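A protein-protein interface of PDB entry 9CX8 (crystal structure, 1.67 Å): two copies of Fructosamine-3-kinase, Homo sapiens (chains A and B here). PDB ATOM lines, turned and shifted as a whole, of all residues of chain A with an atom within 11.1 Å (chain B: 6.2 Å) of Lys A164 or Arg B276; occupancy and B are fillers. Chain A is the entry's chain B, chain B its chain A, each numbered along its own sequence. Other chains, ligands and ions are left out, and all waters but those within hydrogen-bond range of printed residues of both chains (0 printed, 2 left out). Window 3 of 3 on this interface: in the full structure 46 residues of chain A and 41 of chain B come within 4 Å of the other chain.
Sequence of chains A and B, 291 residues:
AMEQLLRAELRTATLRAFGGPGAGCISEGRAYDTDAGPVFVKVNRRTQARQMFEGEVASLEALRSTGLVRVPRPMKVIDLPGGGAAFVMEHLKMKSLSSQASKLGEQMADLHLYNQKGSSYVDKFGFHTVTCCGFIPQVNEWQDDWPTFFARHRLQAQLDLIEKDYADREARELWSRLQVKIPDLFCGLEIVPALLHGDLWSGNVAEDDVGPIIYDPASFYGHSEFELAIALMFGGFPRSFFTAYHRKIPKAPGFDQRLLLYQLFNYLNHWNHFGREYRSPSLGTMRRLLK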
ATOM      1  N   ILE A 136      37.403 -22.346   6.243  1.00  0.00           N
ATOM      2  CA  ILE A 136      36.824 -21.042   6.548  1.00  0.00           C
ATOM      3  C   ILE A 136      37.742 -20.309   7.525  1.00  0.00           C
ATOM      4  O   ILE A 136      37.841 -20.722   8.679  1.00  0.00           O
ATOM      5  CB  ILE A 136      35.401 -21.198   7.111  1.00  0.00           C
ATOM      6  CG1 ILE A 136      34.528 -21.954   6.099  1.00  0.00           C
ATOM      7  CG2 ILE A 136      34.810 -19.872   7.586  1.00  0.00           C
ATOM      8  CD1 ILE A 136      33.101 -22.271   6.634  1.00  0.00           C
ATOM      9  N   PRO A 137      38.369 -19.204   7.123  1.00  0.00           N
ATOM     10  CA  PRO A 137      39.170 -18.418   8.063  1.00  0.00           C
ATOM     11  C   PRO A 137      38.268 -17.864   9.158  1.00  0.00           C
ATOM     12  O   PRO A 137      37.135 -17.442   8.882  1.00  0.00           O
ATOM     13  CB  PRO A 137      39.727 -17.285   7.205  1.00  0.00           C
ATOM     14  CG  PRO A 137      39.546 -17.741   5.752  1.00  0.00           C
ATOM     15  CD  PRO A 137      38.273 -18.575   5.794  1.00  0.00           C
ATOM     16  N   LEU A 155      29.111 -17.965  15.415  1.00  0.00           N
ATOM     17  CA  LEU A 155      27.784 -18.197  14.834  1.00  0.00           C
ATOM     18  C   LEU A 155      27.492 -17.191  13.724  1.00  0.00           C
ATOM     19  O   LEU A 155      27.082 -17.574  12.611  1.00  0.00           O
ATOM     20  CB  LEU A 155      26.677 -18.127  15.891  1.00  0.00           C
ATOM     21  CG  LEU A 155      26.817 -19.277  16.909  1.00  0.00           C
ATOM     22  CD1 LEU A 155      25.838 -19.088  18.110  1.00  0.00           C
ATOM     23  CD2 LEU A 155      26.579 -20.734  16.287  1.00  0.00           C
ATOM     24  N   GLN A 156      27.664 -15.888  14.004  1.00  0.00           N
ATOM     25  CA  GLN A 156      27.304 -14.907  12.966  1.00  0.00           C
ATOM     26  C   GLN A 156      28.147 -15.092  11.714  1.00  0.00           C
ATOM     27  O   GLN A 156      27.651 -14.933  10.582  1.00  0.00           O
ATOM     28  CB  GLN A 156      27.469 -13.489  13.503  1.00  0.00           C
ATOM     29  CG  GLN A 156      27.135 -12.469  12.438  1.00  0.00           C
ATOM     30  CD  GLN A 156      25.657 -12.190  12.405  1.00  0.00           C
ATOM     31  OE1 GLN A 156      25.040 -11.938  13.444  1.00  0.00           O
ATOM     32  NE2 GLN A 156      25.082 -12.173  11.209  1.00  0.00           N
ATOM     33  N   ALA A 157      29.418 -15.399  11.888  1.00  0.00           N
ATOM     34  CA  ALA A 157      30.277 -15.596  10.732  1.00  0.00           C
ATOM     35  C   ALA A 157      29.760 -16.745   9.859  1.00  0.00           C
ATOM     36  O   ALA A 157      29.726 -16.632   8.616  1.00  0.00           O
ATOM     37  CB  ALA A 157      31.728 -15.873  11.213  1.00  0.00           C
ATOM     38  N   GLN A 158      29.338 -17.853  10.507  1.00  0.00           N
ATOM     39  CA  GLN A 158      28.811 -18.968   9.704  1.00  0.00           C
ATOM     40  C   GLN A 158      27.531 -18.551   9.021  1.00  0.00           C
ATOM     41  O   GLN A 158      27.272 -18.922   7.872  1.00  0.00           O
ATOM     42  CB  GLN A 158      28.555 -20.199  10.597  1.00  0.00           C
ATOM     43  CG  GLN A 158      29.905 -20.762  11.212  1.00  0.00           C
ATOM     44  CD  GLN A 158      30.632 -21.641  10.178  1.00  0.00           C
ATOM     45  OE1 GLN A 158      30.018 -22.134   9.218  1.00  0.00           O
ATOM     46  NE2 GLN A 158      31.934 -21.839  10.356  1.00  0.00           N
ATOM     47  N   LEU A 159      26.672 -17.855   9.746  1.00  0.00           N
ATOM     48  CA  LEU A 159      25.363 -17.514   9.163  1.00  0.00           C
ATOM     49  C   LEU A 159      25.480 -16.455   8.082  1.00  0.00           C
ATOM     50  O   LEU A 159      24.639 -16.424   7.154  1.00  0.00           O
ATOM     51  CB  LEU A 159      24.410 -17.090  10.295  1.00  0.00           C
ATOM     52  CG  LEU A 159      23.851 -18.364  10.949  1.00  0.00           C
ATOM     53  CD1 LEU A 159      23.560 -18.143  12.435  1.00  0.00           C
ATOM     54  CD2 LEU A 159      22.610 -18.905  10.254  1.00  0.00           C
ATOM     55  N   ASP A 160      26.476 -15.565   8.165  1.00  0.00           N
ATOM     56  CA  ASP A 160      26.733 -14.627   7.062  1.00  0.00           C
ATOM     57  C   ASP A 160      27.135 -15.363   5.781  1.00  0.00           C
ATOM     58  O   ASP A 160      26.765 -14.940   4.655  1.00  0.00           O
ATOM     59  CB  ASP A 160      27.864 -13.673   7.433  1.00  0.00           C
ATOM     60  CG  ASP A 160      27.413 -12.588   8.428  1.00  0.00           C
ATOM     61  OD1 ASP A 160      26.201 -12.417   8.617  1.00  0.00           O
ATOM     62  OD2 ASP A 160      28.311 -11.898   8.959  1.00  0.00           O
ATOM     63  N   LEU A 161      27.957 -16.404   5.924  1.00  0.00           N
ATOM     64  CA  LEU A 161      28.268 -17.228   4.745  1.00  0.00           C
ATOM     65  C   LEU A 161      27.044 -17.971   4.238  1.00  0.00           C
ATOM     66  O   LEU A 161      26.883 -18.114   3.020  1.00  0.00           O
ATOM     67  CB  LEU A 161      29.414 -18.212   5.046  1.00  0.00           C
ATOM     68  CG  LEU A 161      30.837 -17.720   5.140  1.00  0.00           C
ATOM     69  CD1 LEU A 161      31.706 -18.791   5.811  1.00  0.00           C
ATOM     70  CD2 LEU A 161      31.313 -17.407   3.701  1.00  0.00           C
ATOM     71  N   ILE A 162      26.198 -18.518   5.131  1.00  0.00           N
ATOM     72  CA  ILE A 162      24.955 -19.132   4.666  1.00  0.00           C
ATOM     73  C   ILE A 162      24.092 -18.117   3.925  1.00  0.00           C
ATOM     74  O   ILE A 162      23.481 -18.448   2.899  1.00  0.00           O
ATOM     75  CB  ILE A 162      24.204 -19.781   5.849  1.00  0.00           C
ATOM     76  CG1 ILE A 162      24.955 -21.100   6.210  1.00  0.00           C
ATOM     77  CG2 ILE A 162      22.723 -20.054   5.508  1.00  0.00           C
ATOM     78  CD1 ILE A 162      24.805 -21.419   7.670  1.00  0.00           C
ATOM     79  N   GLU A 163      24.007 -16.876   4.432  1.00  0.00           N
ATOM     80  CA  GLU A 163      23.223 -15.857   3.705  1.00  0.00           C
ATOM     81  C   GLU A 163      23.802 -15.605   2.317  1.00  0.00           C
ATOM     82  O   GLU A 163      23.059 -15.499   1.316  1.00  0.00           O
ATOM     83  CB  GLU A 163      23.198 -14.570   4.522  1.00  0.00           C
ATOM     84  CG  GLU A 163      22.490 -13.407   3.728  1.00  0.00           C
ATOM     85  CD  GLU A 163      21.028 -13.685   3.400  1.00  0.00           C
ATOM     86  OE1 GLU A 163      20.324 -14.634   3.855  1.00  0.00           O
ATOM     87  OE2 GLU A 163      20.496 -12.847   2.627  1.00  0.00           O
ATOM     88  N   LYS A 164      25.119 -15.447   2.248  1.00  0.00           N
ATOM     89  CA  LYS A 164      25.781 -15.153   0.976  1.00  0.00           C
ATOM     90  C   LYS A 164      25.566 -16.287  -0.019  1.00  0.00           C
ATOM     91  O   LYS A 164      25.161 -16.060  -1.171  1.00  0.00           O
ATOM     92  CB  LYS A 164      27.274 -14.945   1.235  1.00  0.00           C
ATOM     93  CG  LYS A 164      28.108 -14.798  -0.041  1.00  0.00           C
ATOM     94  CD  LYS A 164      29.420 -14.099   0.277  1.00  0.00           C
ATOM     95  CE  LYS A 164      30.623 -14.909  -0.185  1.00  0.00           C
ATOM     96  NZ  LYS A 164      30.608 -15.050  -1.689  1.00  0.00           N
ATOM     97  N   ASP A 165      25.738 -17.534   0.427  1.00  0.00           N
ATOM     98  CA  ASP A 165      25.733 -18.628  -0.566  1.00  0.00           C
ATOM     99  C   ASP A 165      24.368 -19.243  -0.812  1.00  0.00           C
ATOM    100  O   ASP A 165      24.098 -19.702  -1.953  1.00  0.00           O
ATOM    101  CB  ASP A 165      26.723 -19.704  -0.116  1.00  0.00           C
ATOM    102  CG  ASP A 165      28.199 -19.227  -0.230  1.00  0.00           C
ATOM    103  OD1 ASP A 165      28.495 -18.239  -0.947  1.00  0.00           O
ATOM    104  OD2 ASP A 165      29.063 -19.836   0.423  1.00  0.00           O
ATOM    105  N   TYR A 166      23.489 -19.285   0.202  1.00  0.00           N
ATOM    106  CA  TYR A 166      22.168 -19.869   0.078  1.00  0.00           C
ATOM    107  C   TYR A 166      21.034 -18.859   0.188  1.00  0.00           C
ATOM    108  O   TYR A 166      19.903 -19.212  -0.138  1.00  0.00           O
ATOM    109  CB  TYR A 166      21.935 -20.965   1.133  1.00  0.00           C
ATOM    110  CG  TYR A 166      22.988 -22.053   1.149  1.00  0.00           C
ATOM    111  CD1 TYR A 166      22.959 -23.117   0.227  1.00  0.00           C
ATOM    112  CD2 TYR A 166      24.034 -22.003   2.038  1.00  0.00           C
ATOM    113  CE1 TYR A 166      23.989 -24.112   0.256  1.00  0.00           C
ATOM    114  CE2 TYR A 166      25.057 -23.015   2.082  1.00  0.00           C
ATOM    115  CZ  TYR A 166      25.006 -24.057   1.158  1.00  0.00           C
ATOM    116  OH  TYR A 166      26.014 -25.027   1.145  1.00  0.00           O
ATOM    117  N   ALA A 167      21.287 -17.673   0.738  1.00  0.00           N
ATOM    118  CA  ALA A 167      20.241 -16.659   0.971  1.00  0.00           C
ATOM    119  C   ALA A 167      18.998 -17.281   1.590  1.00  0.00           C
ATOM    120  O   ALA A 167      17.861 -17.101   1.120  1.00  0.00           O
ATOM    121  CB  ALA A 167      19.902 -15.918  -0.326  1.00  0.00           C
ATOM    122  N   ASP A 168      19.214 -18.010   2.690  1.00  0.00           N
ATOM    123  CA  ASP A 168      18.168 -18.849   3.287  1.00  0.00           C
ATOM    124  C   ASP A 168      17.337 -18.017   4.265  1.00  0.00           C
ATOM    125  O   ASP A 168      17.852 -17.582   5.294  1.00  0.00           O
ATOM    126  CB  ASP A 168      18.771 -20.071   3.987  1.00  0.00           C
ATOM    127  CG  ASP A 168      17.740 -21.058   4.364  1.00  0.00           C
ATOM    128  OD1 ASP A 168      17.062 -20.830   5.364  1.00  0.00           O
ATOM    129  OD2 ASP A 168      17.558 -22.082   3.675  1.00  0.00           O
ATOM    130  N   ARG A 169      16.050 -17.818   3.956  1.00  0.00           N
ATOM    131  CA  ARG A 169      15.230 -16.926   4.779  1.00  0.00           C
ATOM    132  C   ARG A 169      15.005 -17.486   6.181  1.00  0.00           C
ATOM    133  O   ARG A 169      15.084 -16.741   7.189  1.00  0.00           O
ATOM    134  CB  ARG A 169      13.865 -16.697   4.086  1.00  0.00           C
ATOM    135  CG  ARG A 169      12.920 -15.805   4.855  1.00  0.00           C
ATOM    136  CD  ARG A 169      11.474 -16.051   4.387  1.00  0.00           C
ATOM    137  NE  ARG A 169      10.745 -16.737   5.448  1.00  0.00           N
ATOM    138  CZ  ARG A 169      10.524 -18.046   5.483  1.00  0.00           C
ATOM    139  NH1 ARG A 169      10.916 -18.840   4.493  1.00  0.00           N
ATOM    140  NH2 ARG A 169       9.928 -18.576   6.553  1.00  0.00           N
ATOM    141  N   ALA A 171      16.897 -19.495   7.918  1.00  0.00           N
ATOM    142  CA  ALA A 171      18.099 -19.377   8.750  1.00  0.00           C
ATOM    143  C   ALA A 171      18.245 -17.952   9.282  1.00  0.00           C
ATOM    144  O   ALA A 171      18.564 -17.755  10.459  1.00  0.00           O
ATOM    145  CB  ALA A 171      19.377 -19.762   7.962  1.00  0.00           C
ATOM    146  N   ARG A 172      17.990 -16.951   8.424  1.00  0.00           N
ATOM    147  CA  ARG A 172      18.154 -15.546   8.810  1.00  0.00           C
ATOM    148  C   ARG A 172      17.165 -15.182   9.930  1.00  0.00           C
ATOM    149  O   ARG A 172      17.532 -14.529  10.926  1.00  0.00           O
ATOM    150  CB  ARG A 172      17.888 -14.687   7.558  1.00  0.00           C
ATOM    151  CG  ARG A 172      18.599 -13.405   7.401  1.00  0.00           C
ATOM    152  CD  ARG A 172      18.520 -12.972   5.898  1.00  0.00           C
ATOM    153  NE  ARG A 172      17.151 -12.938   5.374  1.00  0.00           N
ATOM    154  CZ  ARG A 172      16.755 -13.489   4.228  1.00  0.00           C
ATOM    155  NH1 ARG A 172      17.592 -14.152   3.438  1.00  0.00           N
ATOM    156  NH2 ARG A 172      15.481 -13.387   3.861  1.00  0.00           N
ATOM    157  N   TRP A 271      26.950 -27.274   7.050  1.00  0.00           N
ATOM    158  CA  TRP A 271      26.134 -26.745   5.957  1.00  0.00           C
ATOM    159  C   TRP A 271      27.006 -25.983   4.990  1.00  0.00           C
ATOM    160  O   TRP A 271      26.924 -26.177   3.753  1.00  0.00           O
ATOM    161  CB  TRP A 271      24.991 -25.889   6.540  1.00  0.00           C
ATOM    162  CG  TRP A 271      23.936 -25.376   5.570  1.00  0.00           C
ATOM    163  CD1 TRP A 271      23.874 -25.524   4.176  1.00  0.00           C
ATOM    164  CD2 TRP A 271      22.834 -24.566   5.937  1.00  0.00           C
ATOM    165  NE1 TRP A 271      22.759 -24.893   3.699  1.00  0.00           N
ATOM    166  CE2 TRP A 271      22.094 -24.286   4.747  1.00  0.00           C
ATOM    167  CE3 TRP A 271      22.365 -24.070   7.182  1.00  0.00           C
ATOM    168  CZ2 TRP A 271      20.926 -23.513   4.744  1.00  0.00           C
ATOM    169  CZ3 TRP A 271      21.197 -23.298   7.178  1.00  0.00           C
ATOM    170  CH2 TRP A 271      20.468 -23.021   5.963  1.00  0.00           C
ATOM    171  N   ASN A 272      27.864 -25.117   5.517  1.00  0.00           N
ATOM    172  CA  ASN A 272      28.748 -24.349   4.658  1.00  0.00           C
ATOM    173  C   ASN A 272      29.722 -25.255   3.887  1.00  0.00           C
ATOM    174  O   ASN A 272      30.005 -25.002   2.705  1.00  0.00           O
ATOM    175  CB  ASN A 272      29.483 -23.292   5.476  1.00  0.00           C
ATOM    176  CG  ASN A 272      28.641 -22.044   5.640  1.00  0.00           C
ATOM    177  OD1 ASN A 272      28.042 -21.573   4.640  1.00  0.00           O
ATOM    178  ND2 ASN A 272      28.588 -21.483   6.882  1.00  0.00           N
ATOM    179  N   GLY A 275      27.127 -28.629   2.299  1.00  0.00           N
ATOM    180  CA  GLY A 275      25.885 -28.383   1.571  1.00  0.00           C
ATOM    181  C   GLY A 275      24.592 -28.682   2.295  1.00  0.00           C
ATOM    182  O   GLY A 275      24.490 -28.872   3.519  1.00  0.00           O
ATOM    183  N   ARG A 276      23.532 -28.672   1.481  1.00  0.00           N
ATOM    184  CA  ARG A 276      22.143 -28.619   1.919  1.00  0.00           C
ATOM    185  C   ARG A 276      21.727 -29.726   2.865  1.00  0.00           C
ATOM    186  O   ARG A 276      20.717 -29.564   3.552  1.00  0.00           O
ATOM    187  CB  ARG A 276      21.188 -28.684   0.695  1.00  0.00           C
ATOM    188  CG  ARG A 276      21.216 -30.075   0.012  1.00  0.00           C
ATOM    189  CD  ARG A 276      20.382 -30.138  -1.323  1.00  0.00           C
ATOM    190  NE  ARG A 276      18.935 -30.030  -1.132  1.00  0.00           N
ATOM    191  CZ  ARG A 276      18.152 -29.050  -1.584  1.00  0.00           C
ATOM    192  NH1 ARG A 276      18.647 -27.988  -2.219  1.00  0.00           N
ATOM    193  NH2 ARG A 276      16.830 -29.142  -1.406  1.00  0.00           N
ATOM    194  N   TYR B 166      15.832 -19.963  -4.843  1.00  0.00           N
ATOM    195  CA  TYR B 166      16.546 -18.754  -5.201  1.00  0.00           C
ATOM    196  C   TYR B 166      15.733 -17.781  -6.018  1.00  0.00           C
ATOM    197  O   TYR B 166      16.176 -16.646  -6.183  1.00  0.00           O
ATOM    198  CB  TYR B 166      17.826 -19.068  -5.997  1.00  0.00           C
ATOM    199  CG  TYR B 166      18.778 -19.903  -5.206  1.00  0.00           C
ATOM    200  CD1 TYR B 166      19.745 -19.304  -4.386  1.00  0.00           C
ATOM    201  CD2 TYR B 166      18.689 -21.269  -5.223  1.00  0.00           C
ATOM    202  CE1 TYR B 166      20.607 -20.057  -3.629  1.00  0.00           C
ATOM    203  CE2 TYR B 166      19.560 -22.061  -4.461  1.00  0.00           C
ATOM    204  CZ  TYR B 166      20.495 -21.433  -3.632  1.00  0.00           C
ATOM    205  OH  TYR B 166      21.375 -22.188  -2.875  1.00  0.00           O
ATOM    206  N   ASP B 168      15.543 -17.353  -9.180  1.00  0.00           N
ATOM    207  CA  ASP B 168      16.567 -16.734 -10.025  1.00  0.00           C
ATOM    208  C   ASP B 168      16.003 -16.444 -11.423  1.00  0.00           C
ATOM    209  O   ASP B 168      15.731 -17.370 -12.208  1.00  0.00           O
ATOM    210  CB  ASP B 168      17.818 -17.609 -10.126  1.00  0.00           C
ATOM    211  CG  ASP B 168      19.001 -16.867 -10.744  1.00  0.00           C
ATOM    212  OD1 ASP B 168      19.063 -16.778 -11.973  1.00  0.00           O
ATOM    213  OD2 ASP B 168      19.899 -16.373 -10.029  1.00  0.00           O
ATOM    214  N   TRP B 271      24.789 -26.154  -7.654  1.00  0.00           N
ATOM    215  CA  TRP B 271      24.106 -24.942  -7.150  1.00  0.00           C
ATOM    216  C   TRP B 271      23.042 -25.308  -6.106  1.00  0.00           C
ATOM    217  O   TRP B 271      22.992 -24.707  -5.022  1.00  0.00           O
ATOM    218  CB  TRP B 271      23.505 -24.188  -8.356  1.00  0.00           C
ATOM    219  CG  TRP B 271      22.853 -22.862  -8.094  1.00  0.00           C
ATOM    220  CD1 TRP B 271      22.646 -22.235  -6.868  1.00  0.00           C
ATOM    221  CD2 TRP B 271      22.284 -21.997  -9.087  1.00  0.00           C
ATOM    222  NE1 TRP B 271      21.962 -21.010  -7.068  1.00  0.00           N
ATOM    223  CE2 TRP B 271      21.761 -20.847  -8.421  1.00  0.00           C
ATOM    224  CE3 TRP B 271      22.150 -22.090 -10.488  1.00  0.00           C
ATOM    225  CZ2 TRP B 271      21.096 -19.828  -9.107  1.00  0.00           C
ATOM    226  CZ3 TRP B 271      21.536 -21.049 -11.161  1.00  0.00           C
ATOM    227  CH2 TRP B 271      21.024 -19.927 -10.470  1.00  0.00           C
ATOM    228  N   PHE B 274      25.256 -26.661  -2.937  1.00  0.00           N
ATOM    229  CA  PHE B 274      26.322 -25.837  -2.354  1.00  0.00           C
ATOM    230  C   PHE B 274      26.083 -24.343  -2.479  1.00  0.00           C
ATOM    231  O   PHE B 274      26.852 -23.560  -1.896  1.00  0.00           O
ATOM    232  CB  PHE B 274      27.701 -26.186  -2.986  1.00  0.00           C
ATOM    233  CG  PHE B 274      28.064 -27.613  -2.800  1.00  0.00           C
ATOM    234  CD1 PHE B 274      28.318 -28.084  -1.532  1.00  0.00           C
ATOM    235  CD2 PHE B 274      28.146 -28.493  -3.864  1.00  0.00           C
ATOM    236  CE1 PHE B 274      28.611 -29.433  -1.327  1.00  0.00           C
ATOM    237  CE2 PHE B 274      28.459 -29.808  -3.674  1.00  0.00           C
ATOM    238  CZ  PHE B 274      28.688 -30.289  -2.410  1.00  0.00           C
ATOM    239  N   GLY B 275      25.064 -23.921  -3.210  1.00  0.00           N
ATOM    240  CA  GLY B 275      24.754 -22.511  -3.315  1.00  0.00           C
ATOM    241  C   GLY B 275      25.366 -21.767  -4.488  1.00  0.00           C
ATOM    242  O   GLY B 275      25.808 -22.319  -5.514  1.00  0.00           O
ATOM    243  N   ARG B 276      25.431 -20.448  -4.293  1.00  0.00           N
ATOM    244  CA  ARG B 276      25.572 -19.530  -5.415  1.00  0.00           C
ATOM    245  C   ARG B 276      26.941 -19.541  -6.061  1.00  0.00           C
ATOM    246  O   ARG B 276      27.070 -18.968  -7.155  1.00  0.00           O
ATOM    247  CB  ARG B 276      25.200 -18.093  -4.974  1.00  0.00           C
ATOM    248  CG  ARG B 276      23.675 -17.902  -4.794  1.00  0.00           C
ATOM    249  CD  ARG B 276      23.303 -16.403  -4.561  1.00  0.00           C
ATOM    250  NE  ARG B 276      24.169 -15.503  -5.332  1.00  0.00           N
ATOM    251  CZ  ARG B 276      23.787 -14.791  -6.392  1.00  0.00           C
ATOM    252  NH1 ARG B 276      22.522 -14.754  -6.791  1.00  0.00           N
ATOM    253  NH2 ARG B 276      24.697 -14.097  -7.073  1.00  0.00           N
ATOM    254  N   GLU B 277      27.955 -20.160  -5.452  1.00  0.00           N
ATOM    255  CA  GLU B 277      29.228 -20.335  -6.133  1.00  0.00           C
ATOM    256  C   GLU B 277      28.995 -21.002  -7.490  1.00  0.00           C
ATOM    257  O   GLU B 277      29.743 -20.750  -8.444  1.00  0.00           O
ATOM    258  CB  GLU B 277      30.170 -21.196  -5.292  1.00  0.00           C
ATOM    259  CG  GLU B 277      31.430 -21.730  -6.031  1.00  0.00           C
ATOM    260  CD  GLU B 277      32.268 -22.779  -5.231  1.00  0.00           C
ATOM    261  OE1 GLU B 277      31.867 -23.228  -4.117  1.00  0.00           O
ATOM    262  OE2 GLU B 277      33.320 -23.204  -5.767  1.00  0.00           O
ATOM    263  N   TYR B 278      27.959 -21.828  -7.589  1.00  0.00           N
ATOM    264  CA  TYR B 278      27.679 -22.540  -8.847  1.00  0.00           C
ATOM    265  C   TYR B 278      26.656 -21.876  -9.748  1.00  0.00           C
ATOM    266  O   TYR B 278      26.352 -22.435 -10.820  1.00  0.00           O
ATOM    267  CB  TYR B 278      27.284 -24.005  -8.557  1.00  0.00           C
ATOM    268  CG  TYR B 278      28.434 -24.752  -8.018  1.00  0.00           C
ATOM    269  CD1 TYR B 278      29.401 -25.277  -8.888  1.00  0.00           C
ATOM    270  CD2 TYR B 278      28.596 -24.918  -6.641  1.00  0.00           C
ATOM    271  CE1 TYR B 278      30.514 -25.931  -8.400  1.00  0.00           C
ATOM    272  CE2 TYR B 278      29.677 -25.596  -6.146  1.00  0.00           C
ATOM    273  CZ  TYR B 278      30.639 -26.092  -7.019  1.00  0.00           C
ATOM    274  OH  TYR B 278      31.714 -26.747  -6.517  1.00  0.00           O
ATOM    275  N   ARG B 279      26.212 -20.646  -9.432  1.00  0.00           N
ATOM    276  CA  ARG B 279      25.273 -19.952 -10.325  1.00  0.00           C
ATOM    277  C   ARG B 279      25.969 -19.542 -11.613  1.00  0.00           C
ATOM    278  O   ARG B 279      25.449 -19.759 -12.716  1.00  0.00           O
ATOM    279  CB  ARG B 279      24.687 -18.715  -9.611  1.00  0.00           C
ATOM    280  CG  ARG B 279      23.847 -17.806 -10.486  1.00  0.00           C
ATOM    281  CD  ARG B 279      23.286 -16.572  -9.681  1.00  0.00           C
ATOM    282  NE  ARG B 279      22.389 -15.776 -10.526  1.00  0.00           N
ATOM    283  CZ  ARG B 279      22.819 -14.761 -11.264  1.00  0.00           C
ATOM    284  NH1 ARG B 279      24.099 -14.422 -11.282  1.00  0.00           N
ATOM    285  NH2 ARG B 279      21.966 -14.127 -12.067  1.00  0.00           N
ATOM    286  N   SER B 280      27.186 -18.988 -11.488  1.00  0.00           N
ATOM    287  CA  SER B 280      27.882 -18.495 -12.680  1.00  0.00           C
ATOM    288  C   SER B 280      28.169 -19.606 -13.717  1.00  0.00           C
ATOM    289  O   SER B 280      27.876 -19.385 -14.904  1.00  0.00           O
ATOM    290  CB  SER B 280      29.162 -17.780 -12.256  1.00  0.00           C
ATOM    291  OG  SER B 280      29.974 -17.557 -13.384  1.00  0.00           O
ATOM    292  N   PRO B 281      28.695 -20.794 -13.354  1.00  0.00           N
ATOM    293  CA  PRO B 281      28.857 -21.858 -14.384  1.00  0.00           C
ATOM    294  C   PRO B 281      27.532 -22.325 -14.916  1.00  0.00           C
ATOM    295  O   PRO B 281      27.437 -22.665 -16.114  1.00  0.00           O
ATOM    296  CB  PRO B 281      29.494 -23.014 -13.610  1.00  0.00           C
ATOM    297  CG  PRO B 281      30.117 -22.418 -12.436  1.00  0.00           C
ATOM    298  CD  PRO B 281      29.242 -21.256 -12.066  1.00  0.00           C
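Pro A137 touches none of the printed residues of chain B. Lys A164 touches one residue of chain B. Of the printed residues of chain B, Asp A165 touches Tyr B166 (3.8 Å), Gly B275 (3.2 Å) and Arg B276 (2.8 Å). Printed residues of chain B within 4 Å of Gly A275: Phe B274 (3.95 Å). Printed residues of chain A within 4 Å of Tyr B166: Asp A165 (3.8 Å) and Tyr A166 (3.6 Å). Printed residues of chain A within 4 Å of Phe B274: Tyr A166 and Gly A275. Gly B275 touches just these residues of chain A: Asp A165 and Tyr A166. Arg B276 touches just these residues of chain A: Lys A164 (3.9 Å) and Asp A165 (2.8 Å). No residue of chain A comes within 4 Å of Arg B279. Ser B280 touches none of the printed residues of chain A. The nearest printed residue of chain B that does not touch Lys A164 is Tyr B166 (6.5 Å). The nearest residue of chain A that does not touch Arg B276 is Tyr A166 (5.0 Å). The nearest printed residue of chain B that does not touch Asp A165 is Phe B274 (4.2 Å).
Of the 11 printed residues of chain B, 4 touch a printed residue of chain A. Hydrophobic or aromatic side chains of chain B within 4 Å of the printed part of chain A: Tyr B166 and Phe B274. Of the 23 printed residues of chain A, 4 touch a printed residue of chain B. Hydrophobic or aromatic side chains of chain A within 4 Å of the printed part of chain B: Tyr A166. Among the printed residues, no Asp or Glu carboxylate lies within 4 Å of a Lys or Arg side-chain nitrogen of the other chain.
Lys A164 touches Arg B276 (O to CD, 3.9 Å). Asp A165 touches Tyr B166. O of Asp A165 touches CA of Gly B275, at 3.2 Å. Tyr B166 touches Tyr A166. Tyr A166 touches Gly B275. Phe B274 touches Gly A275.
Tyr B166 touches its own counterpart, Tyr A166. Tyr A166 touches Gly B275, but with the chains exchanged Gly A275 does not touch Tyr B166 (8.9 Å).
The backbone carbonyl oxygen (O) of Trp A271 lies within hydrogen-bond range of the side-chain hydroxyl (OH) of Tyr A166, at 3.0 Å. NZ of Lys A164 lies within salt-bridge range of OD1 of Asp A165 (3.9 Å).
The backbone NH (N) of Arg B276 lies within hydrogen-bond range of the backbone carbonyl oxygen (O) of Asp A165 (2.8 Å). The backbone carbonyl oxygen of Phe B274 is in hydrogen-bond range of the side-chain hydroxyl of Tyr A166 (3.5 Å).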
